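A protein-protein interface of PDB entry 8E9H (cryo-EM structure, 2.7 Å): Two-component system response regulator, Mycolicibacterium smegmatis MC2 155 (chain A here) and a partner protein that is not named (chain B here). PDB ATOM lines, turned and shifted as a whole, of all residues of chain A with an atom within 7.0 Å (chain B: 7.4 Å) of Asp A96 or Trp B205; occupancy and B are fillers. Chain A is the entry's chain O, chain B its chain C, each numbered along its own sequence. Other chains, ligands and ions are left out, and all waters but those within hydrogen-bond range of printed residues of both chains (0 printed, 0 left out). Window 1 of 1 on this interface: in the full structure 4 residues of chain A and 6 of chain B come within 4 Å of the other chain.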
ATOM      1  N   THR A  92     -25.987  13.788   7.047  1.00  0.00           N
ATOM      2  CA  THR A  92     -24.980  14.836   6.987  1.00  0.00           C
ATOM      3  C   THR A  92     -25.295  15.905   8.021  1.00  0.00           C
ATOM      4  O   THR A  92     -26.452  16.310   8.168  1.00  0.00           O
ATOM      5  CB  THR A  92     -24.920  15.460   5.595  1.00  0.00           C
ATOM      6  OG1 THR A  92     -26.182  16.059   5.282  1.00  0.00           O
ATOM      7  CG2 THR A  92     -24.600  14.405   4.557  1.00  0.00           C
ATOM      8  N   GLY A  93     -24.264  16.361   8.729  1.00  0.00           N
ATOM      9  CA  GLY A  93     -24.449  17.340   9.783  1.00  0.00           C
ATOM     10  C   GLY A  93     -24.605  18.767   9.301  1.00  0.00           C
ATOM     11  O   GLY A  93     -24.911  19.641  10.118  1.00  0.00           O
ATOM     12  N   ARG A  94     -24.400  19.028   8.015  1.00  0.00           N
ATOM     13  CA  ARG A  94     -24.546  20.380   7.498  1.00  0.00           C
ATOM     14  C   ARG A  94     -24.730  20.322   5.992  1.00  0.00           C
ATOM     15  O   ARG A  94     -24.446  19.309   5.351  1.00  0.00           O
ATOM     16  CB  ARG A  94     -23.340  21.249   7.852  1.00  0.00           C
ATOM     17  CG  ARG A  94     -22.013  20.579   7.600  1.00  0.00           C
ATOM     18  CD  ARG A  94     -20.894  21.591   7.563  1.00  0.00           C
ATOM     19  NE  ARG A  94     -19.597  20.955   7.393  1.00  0.00           N
ATOM     20  CZ  ARG A  94     -18.468  21.610   7.170  1.00  0.00           C
ATOM     21  NH1 ARG A  94     -18.437  22.929   7.100  1.00  0.00           N
ATOM     22  NH2 ARG A  94     -17.343  20.924   7.010  1.00  0.00           N
ATOM     23  N   ALA A  95     -25.211  21.433   5.435  1.00  0.00           N
ATOM     24  CA  ALA A  95     -25.435  21.497   3.997  1.00  0.00           C
ATOM     25  C   ALA A  95     -24.130  21.343   3.231  1.00  0.00           C
ATOM     26  O   ALA A  95     -24.073  20.628   2.226  1.00  0.00           O
ATOM     27  CB  ALA A  95     -26.115  22.814   3.631  1.00  0.00           C
ATOM     28  N   ASP A  96     -23.071  22.002   3.691  1.00  0.00           N
ATOM     29  CA  ASP A  96     -21.804  21.955   2.976  1.00  0.00           C
ATOM     30  C   ASP A  96     -21.170  20.576   2.987  1.00  0.00           C
ATOM     31  O   ASP A  96     -20.238  20.342   2.212  1.00  0.00           O
ATOM     32  CB  ASP A  96     -20.838  22.977   3.566  1.00  0.00           C
ATOM     33  CG  ASP A  96     -21.369  24.388   3.474  1.00  0.00           C
ATOM     34  OD1 ASP A  96     -22.194  24.770   4.329  1.00  0.00           O
ATOM     35  OD2 ASP A  96     -20.969  25.114   2.541  1.00  0.00           O
ATOM     36  N   ASP A  97     -21.635  19.663   3.832  1.00  0.00           N
ATOM     37  CA  ASP A  97     -21.177  18.284   3.779  1.00  0.00           C
ATOM     38  C   ASP A  97     -21.686  17.550   2.551  1.00  0.00           C
ATOM     39  O   ASP A  97     -21.181  16.466   2.242  1.00  0.00           O
ATOM     40  CB  ASP A  97     -21.619  17.529   5.035  1.00  0.00           C
ATOM     41  CG  ASP A  97     -20.603  17.613   6.158  1.00  0.00           C
ATOM     42  OD1 ASP A  97     -19.415  17.881   5.879  1.00  0.00           O
ATOM     43  OD2 ASP A  97     -20.991  17.407   7.326  1.00  0.00           O
ATOM     44  N   ALA A  98     -22.653  18.125   1.833  1.00  0.00           N
ATOM     45  CA  ALA A  98     -23.220  17.448   0.675  1.00  0.00           C
ATOM     46  C   ALA A  98     -22.138  16.973  -0.277  1.00  0.00           C
ATOM     47  O   ALA A  98     -22.195  15.841  -0.768  1.00  0.00           O
ATOM     48  CB  ALA A  98     -24.186  18.381  -0.053  1.00  0.00           C
ATOM     49  N   TRP A  99     -21.136  17.811  -0.538  1.00  0.00           N
ATOM     50  CA  TRP A  99     -20.059  17.400  -1.428  1.00  0.00           C
ATOM     51  C   TRP A  99     -19.432  16.096  -0.960  1.00  0.00           C
ATOM     52  O   TRP A  99     -19.338  15.136  -1.731  1.00  0.00           O
ATOM     53  CB  TRP A  99     -19.007  18.500  -1.511  1.00  0.00           C
ATOM     54  CG  TRP A  99     -17.999  18.272  -2.575  1.00  0.00           C
ATOM     55  CD1 TRP A  99     -18.137  18.540  -3.901  1.00  0.00           C
ATOM     56  CD2 TRP A  99     -16.687  17.735  -2.408  1.00  0.00           C
ATOM     57  NE1 TRP A  99     -16.992  18.199  -4.573  1.00  0.00           N
ATOM     58  CE2 TRP A  99     -16.086  17.702  -3.675  1.00  0.00           C
ATOM     59  CE3 TRP A  99     -15.963  17.276  -1.307  1.00  0.00           C
ATOM     60  CZ2 TRP A  99     -14.795  17.231  -3.875  1.00  0.00           C
ATOM     61  CZ3 TRP A  99     -14.684  16.809  -1.507  1.00  0.00           C
ATOM     62  CH2 TRP A  99     -14.112  16.789  -2.779  1.00  0.00           C
ATOM     63  N   LEU A 100     -19.032  16.023   0.310  1.00  0.00           N
ATOM     64  CA  LEU A 100     -18.472  14.774   0.806  1.00  0.00           C
ATOM     65  C   LEU A 100     -19.484  13.646   0.726  1.00  0.00           C
ATOM     66  O   LEU A 100     -19.106  12.497   0.474  1.00  0.00           O
ATOM     67  CB  LEU A 100     -17.984  14.930   2.240  1.00  0.00           C
ATOM     68  CG  LEU A 100     -16.643  15.627   2.440  1.00  0.00           C
ATOM     69  CD1 LEU A 100     -16.305  15.676   3.913  1.00  0.00           C
ATOM     70  CD2 LEU A 100     -15.551  14.915   1.675  1.00  0.00           C
ATOM     71  N   ALA A 101     -20.766  13.943   0.932  1.00  0.00           N
ATOM     72  CA  ALA A 101     -21.775  12.903   0.781  1.00  0.00           C
ATOM     73  C   ALA A 101     -21.705  12.294  -0.608  1.00  0.00           C
ATOM     74  O   ALA A 101     -21.865  11.080  -0.771  1.00  0.00           O
ATOM     75  CB  ALA A 101     -23.165  13.471   1.051  1.00  0.00           C
ATOM     76  N   ASP B 184     -13.848  31.886  -8.323  1.00  0.00           N
ATOM     77  CA  ASP B 184     -14.257  30.799  -7.447  1.00  0.00           C
ATOM     78  C   ASP B 184     -14.996  31.333  -6.232  1.00  0.00           C
ATOM     79  O   ASP B 184     -16.032  30.795  -5.832  1.00  0.00           O
ATOM     80  CB  ASP B 184     -13.035  29.994  -7.014  1.00  0.00           C
ATOM     81  CG  ASP B 184     -13.405  28.655  -6.425  1.00  0.00           C
ATOM     82  OD1 ASP B 184     -14.613  28.380  -6.294  1.00  0.00           O
ATOM     83  OD2 ASP B 184     -12.490  27.879  -6.087  1.00  0.00           O
ATOM     84  N   ARG B 198     -12.435  26.875 -11.438  1.00  0.00           N
ATOM     85  CA  ARG B 198     -12.224  26.967 -10.005  1.00  0.00           C
ATOM     86  C   ARG B 198     -10.828  26.472  -9.649  1.00  0.00           C
ATOM     87  O   ARG B 198     -10.309  25.518 -10.232  1.00  0.00           O
ATOM     88  CB  ARG B 198     -13.272  26.152  -9.254  1.00  0.00           C
ATOM     89  CG  ARG B 198     -14.652  26.759  -9.282  1.00  0.00           C
ATOM     90  CD  ARG B 198     -15.592  26.011  -8.368  1.00  0.00           C
ATOM     91  NE  ARG B 198     -16.956  26.515  -8.462  1.00  0.00           N
ATOM     92  CZ  ARG B 198     -17.500  27.385  -7.621  1.00  0.00           C
ATOM     93  NH1 ARG B 198     -16.823  27.879  -6.599  1.00  0.00           N
ATOM     94  NH2 ARG B 198     -18.756  27.771  -7.814  1.00  0.00           N
ATOM     95  N   GLU B 200      -9.608  26.982  -5.989  1.00  0.00           N
ATOM     96  CA  GLU B 200      -9.659  26.600  -4.584  1.00  0.00           C
ATOM     97  C   GLU B 200     -10.732  25.550  -4.318  1.00  0.00           C
ATOM     98  O   GLU B 200     -10.428  24.458  -3.830  1.00  0.00           O
ATOM     99  CB  GLU B 200      -9.907  27.838  -3.722  1.00  0.00           C
ATOM    100  CG  GLU B 200      -8.770  28.839  -3.752  1.00  0.00           C
ATOM    101  CD  GLU B 200      -7.576  28.388  -2.955  1.00  0.00           C
ATOM    102  OE1 GLU B 200      -7.620  27.273  -2.402  1.00  0.00           O
ATOM    103  OE2 GLU B 200      -6.593  29.151  -2.875  1.00  0.00           O
ATOM    104  N   MET B 201     -11.981  25.863  -4.629  1.00  0.00           N
ATOM    105  CA  MET B 201     -13.075  24.924  -4.459  1.00  0.00           C
ATOM    106  C   MET B 201     -13.020  23.808  -5.493  1.00  0.00           C
ATOM    107  O   MET B 201     -12.473  23.983  -6.583  1.00  0.00           O
ATOM    108  CB  MET B 201     -14.408  25.653  -4.575  1.00  0.00           C
ATOM    109  CG  MET B 201     -14.648  26.663  -3.493  1.00  0.00           C
ATOM    110  SD  MET B 201     -14.896  25.784  -1.947  1.00  0.00           S
ATOM    111  CE  MET B 201     -13.411  26.225  -1.089  1.00  0.00           C
ATOM    112  N   PRO B 202     -13.587  22.646  -5.175  1.00  0.00           N
ATOM    113  CA  PRO B 202     -13.746  21.614  -6.198  1.00  0.00           C
ATOM    114  C   PRO B 202     -14.594  22.130  -7.346  1.00  0.00           C
ATOM    115  O   PRO B 202     -15.520  22.919  -7.156  1.00  0.00           O
ATOM    116  CB  PRO B 202     -14.448  20.476  -5.451  1.00  0.00           C
ATOM    117  CG  PRO B 202     -14.146  20.713  -4.029  1.00  0.00           C
ATOM    118  CD  PRO B 202     -14.076  22.192  -3.865  1.00  0.00           C
ATOM    119  N   ASP B 203     -14.266  21.676  -8.555  1.00  0.00           N
ATOM    120  CA  ASP B 203     -15.045  22.091  -9.714  1.00  0.00           C
ATOM    121  C   ASP B 203     -16.510  21.731  -9.546  1.00  0.00           C
ATOM    122  O   ASP B 203     -17.382  22.381 -10.131  1.00  0.00           O
ATOM    123  CB  ASP B 203     -14.484  21.447 -10.977  1.00  0.00           C
ATOM    124  CG  ASP B 203     -13.097  21.936 -11.303  1.00  0.00           C
ATOM    125  OD1 ASP B 203     -12.151  21.551 -10.588  1.00  0.00           O
ATOM    126  OD2 ASP B 203     -12.952  22.710 -12.269  1.00  0.00           O
ATOM    127  N   ASP B 204     -16.799  20.710  -8.743  1.00  0.00           N
ATOM    128  CA  ASP B 204     -18.170  20.299  -8.484  1.00  0.00           C
ATOM    129  C   ASP B 204     -18.849  21.153  -7.424  1.00  0.00           C
ATOM    130  O   ASP B 204     -20.045  20.972  -7.182  1.00  0.00           O
ATOM    131  CB  ASP B 204     -18.182  18.835  -8.053  1.00  0.00           C
ATOM    132  CG  ASP B 204     -19.570  18.249  -8.025  1.00  0.00           C
ATOM    133  OD1 ASP B 204     -20.443  18.755  -8.756  1.00  0.00           O
ATOM    134  OD2 ASP B 204     -19.788  17.277  -7.276  1.00  0.00           O
ATOM    135  N   TRP B 205     -18.126  22.072  -6.795  1.00  0.00           N
ATOM    136  CA  TRP B 205     -18.695  22.854  -5.710  1.00  0.00           C
ATOM    137  C   TRP B 205     -19.840  23.721  -6.207  1.00  0.00           C
ATOM    138  O   TRP B 205     -19.855  24.176  -7.353  1.00  0.00           O
ATOM    139  CB  TRP B 205     -17.628  23.736  -5.072  1.00  0.00           C
ATOM    140  CG  TRP B 205     -17.983  24.185  -3.699  1.00  0.00           C
ATOM    141  CD1 TRP B 205     -18.509  25.387  -3.341  1.00  0.00           C
ATOM    142  CD2 TRP B 205     -17.841  23.434  -2.491  1.00  0.00           C
ATOM    143  NE1 TRP B 205     -18.702  25.434  -1.985  1.00  0.00           N
ATOM    144  CE2 TRP B 205     -18.299  24.245  -1.440  1.00  0.00           C
ATOM    145  CE3 TRP B 205     -17.370  22.154  -2.198  1.00  0.00           C
ATOM    146  CZ2 TRP B 205     -18.299  23.819  -0.120  1.00  0.00           C
ATOM    147  CZ3 TRP B 205     -17.370  21.735  -0.888  1.00  0.00           C
ATOM    148  CH2 TRP B 205     -17.831  22.564   0.135  1.00  0.00           C
ATOM    149  N   GLU B 206     -20.807  23.949  -5.327  1.00  0.00           N
ATOM    150  CA  GLU B 206     -21.952  24.798  -5.616  1.00  0.00           C
ATOM    151  C   GLU B 206     -21.837  26.084  -4.811  1.00  0.00           C
ATOM    152  O   GLU B 206     -21.641  26.043  -3.593  1.00  0.00           O
ATOM    153  CB  GLU B 206     -23.258  24.079  -5.281  1.00  0.00           C
ATOM    154  N   GLY B 207     -21.965  27.219  -5.493  1.00  0.00           N
ATOM    155  CA  GLY B 207     -21.891  28.505  -4.836  1.00  0.00           C
ATOM    156  C   GLY B 207     -20.487  29.070  -4.819  1.00  0.00           C
ATOM    157  O   GLY B 207     -19.502  28.413  -5.154  1.00  0.00           O
ATOM    158  N   HIS B 208     -20.404  30.334  -4.413  1.00  0.00           N
ATOM    159  CA  HIS B 208     -19.145  31.075  -4.376  1.00  0.00           C
ATOM    160  C   HIS B 208     -18.903  31.534  -2.945  1.00  0.00           C
ATOM    161  O   HIS B 208     -19.521  32.514  -2.493  1.00  0.00           O
ATOM    162  CB  HIS B 208     -19.187  32.247  -5.342  1.00  0.00           C
ATOM    163  CG  HIS B 208     -19.340  31.831  -6.769  1.00  0.00           C
ATOM    164  ND1 HIS B 208     -18.375  31.110  -7.438  1.00  0.00           N
ATOM    165  CD2 HIS B 208     -20.348  32.019  -7.650  1.00  0.00           C
ATOM    166  CE1 HIS B 208     -18.780  30.878  -8.673  1.00  0.00           C
ATOM    167  NE2 HIS B 208     -19.973  31.421  -8.829  1.00  0.00           N
ATOM    168  N   PRO B 209     -18.013  30.869  -2.207  1.00  0.00           N
ATOM    169  CA  PRO B 209     -18.046  31.002  -0.742  1.00  0.00           C
ATOM    170  C   PRO B 209     -17.934  32.418  -0.208  1.00  0.00           C
ATOM    171  O   PRO B 209     -18.637  32.753   0.751  1.00  0.00           O
ATOM    172  CB  PRO B 209     -16.857  30.147  -0.300  1.00  0.00           C
ATOM    173  CG  PRO B 209     -16.677  29.164  -1.371  1.00  0.00           C
ATOM    174  CD  PRO B 209     -17.042  29.852  -2.639  1.00  0.00           C
ATOM    175  N   TYR B 214     -23.502  33.877   0.800  1.00  0.00           N
ATOM    176  CA  TYR B 214     -23.126  32.487   1.011  1.00  0.00           C
ATOM    177  C   TYR B 214     -22.934  32.228   2.500  1.00  0.00           C
ATOM    178  O   TYR B 214     -22.106  32.899   3.130  1.00  0.00           O
ATOM    179  CB  TYR B 214     -21.849  32.177   0.250  1.00  0.00           C
ATOM    180  CG  TYR B 214     -21.495  30.714   0.199  1.00  0.00           C
ATOM    181  CD1 TYR B 214     -20.862  30.096   1.263  1.00  0.00           C
ATOM    182  CD2 TYR B 214     -21.778  29.954  -0.921  1.00  0.00           C
ATOM    183  CE1 TYR B 214     -20.530  28.765   1.215  1.00  0.00           C
ATOM    184  CE2 TYR B 214     -21.449  28.621  -0.977  1.00  0.00           C
ATOM    185  CZ  TYR B 214     -20.826  28.032   0.094  1.00  0.00           C
ATOM    186  OH  TYR B 214     -20.497  26.701   0.043  1.00  0.00           O
ATOM    187  N   PRO B 215     -23.645  31.279   3.099  1.00  0.00           N
ATOM    188  CA  PRO B 215     -23.527  31.076   4.544  1.00  0.00           C
ATOM    189  C   PRO B 215     -22.159  30.536   4.931  1.00  0.00           C
ATOM    190  O   PRO B 215     -21.465  29.888   4.147  1.00  0.00           O
ATOM    191  CB  PRO B 215     -24.631  30.063   4.850  1.00  0.00           C
ATOM    192  CG  PRO B 215     -24.798  29.315   3.590  1.00  0.00           C
ATOM    193  CD  PRO B 215     -24.558  30.299   2.487  1.00  0.00           C
ATOM    194  N   LEU B 216     -21.779  30.816   6.178  1.00  0.00           N
ATOM    195  CA  LEU B 216     -20.475  30.386   6.665  1.00  0.00           C
ATOM    196  C   LEU B 216     -20.319  28.875   6.605  1.00  0.00           C
ATOM    197  O   LEU B 216     -19.205  28.376   6.419  1.00  0.00           O
ATOM    198  CB  LEU B 216     -20.263  30.875   8.094  1.00  0.00           C
ATOM    199  CG  LEU B 216     -18.881  30.612   8.686  1.00  0.00           C
ATOM    200  CD1 LEU B 216     -17.816  31.347   7.905  1.00  0.00           C
ATOM    201  CD2 LEU B 216     -18.852  31.019  10.139  1.00  0.00           C
ATOM    202  N   GLY B 217     -21.409  28.133   6.769  1.00  0.00           N
ATOM    203  CA  GLY B 217     -21.344  26.693   6.639  1.00  0.00           C
ATOM    204  C   GLY B 217     -20.696  25.976   7.797  1.00  0.00           C
ATOM    205  O   GLY B 217     -20.209  24.858   7.623  1.00  0.00           O
ATOM    206  N   GLY B 218     -20.674  26.581   8.977  1.00  0.00           N
ATOM    207  CA  GLY B 218     -20.133  25.923  10.143  1.00  0.00           C
ATOM    208  C   GLY B 218     -21.119  24.939  10.739  1.00  0.00           C
ATOM    209  O   GLY B 218     -22.242  24.759  10.269  1.00  0.00           O
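Trp B205 touches Asp A96 (CH2 to O, 3.9 Å). Asp A96 touches Gly B217 (OD1 to CA, 3.1 Å). NE1 of Trp A99 touches CB of Pro B202 (3.5 Å). Asp B204 touches Trp A99. Trp A99 touches Trp B205 (CB to CZ3, 3.7 Å).
OD1 of Asp A97 lies within salt-bridge range of NE of Arg A94 (3.4 Å). OH of Tyr B214 is in hydrogen-bond range of NE1 of Trp B205, at 3.0 Å.
Of the 17 printed residues of chain B, 5 touch a printed residue of chain A. Hydrophobic or aromatic side chains of chain A that line the printed part of chain B: Trp A99. Among the printed residues, 7 pairs touch across the chains.
No residue of chain B comes within 4 Å of Ala A95. Asp A96 touches just these residues of chain B: Trp B205 (3.9 Å), Tyr B214 (3.0 Å) and Gly B217 (3.1 Å). Of the printed residues of chain B, Trp A99 touches Pro B202 (3.5 Å), Asp B204 (3.7 Å) and Trp B205 (3.7 Å). Printed residues of chain A within 4 Å of Pro B202: Trp A99. Of the printed residues of chain A, Asp B204 touches Trp A99. Trp B205 touches just these residues of chain A: Asp A96 (3.9 Å) and Trp A99 (3.7 Å). Of the printed residues of chain A, Tyr B214 touches Asp A96. Of the printed residues of chain A, Gly B217 touches Arg A94 (2.7 Å) and Asp A96 (3.1 Å). The nearest printed residue of chain B that does not touch Asp A96 is Leu B216 (5.1 Å). The nearest printed residue of chain B that does not touch Arg A94 is Gly B218 (4.4 Å).
NH1 of Arg A94 is in hydrogen-bond range of O of Gly B217. The side-chain hydroxyl of Tyr B214 sits at hydrogen-bond distance from the side-chain carboxylate of Asp A96, 3.0 Å away.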
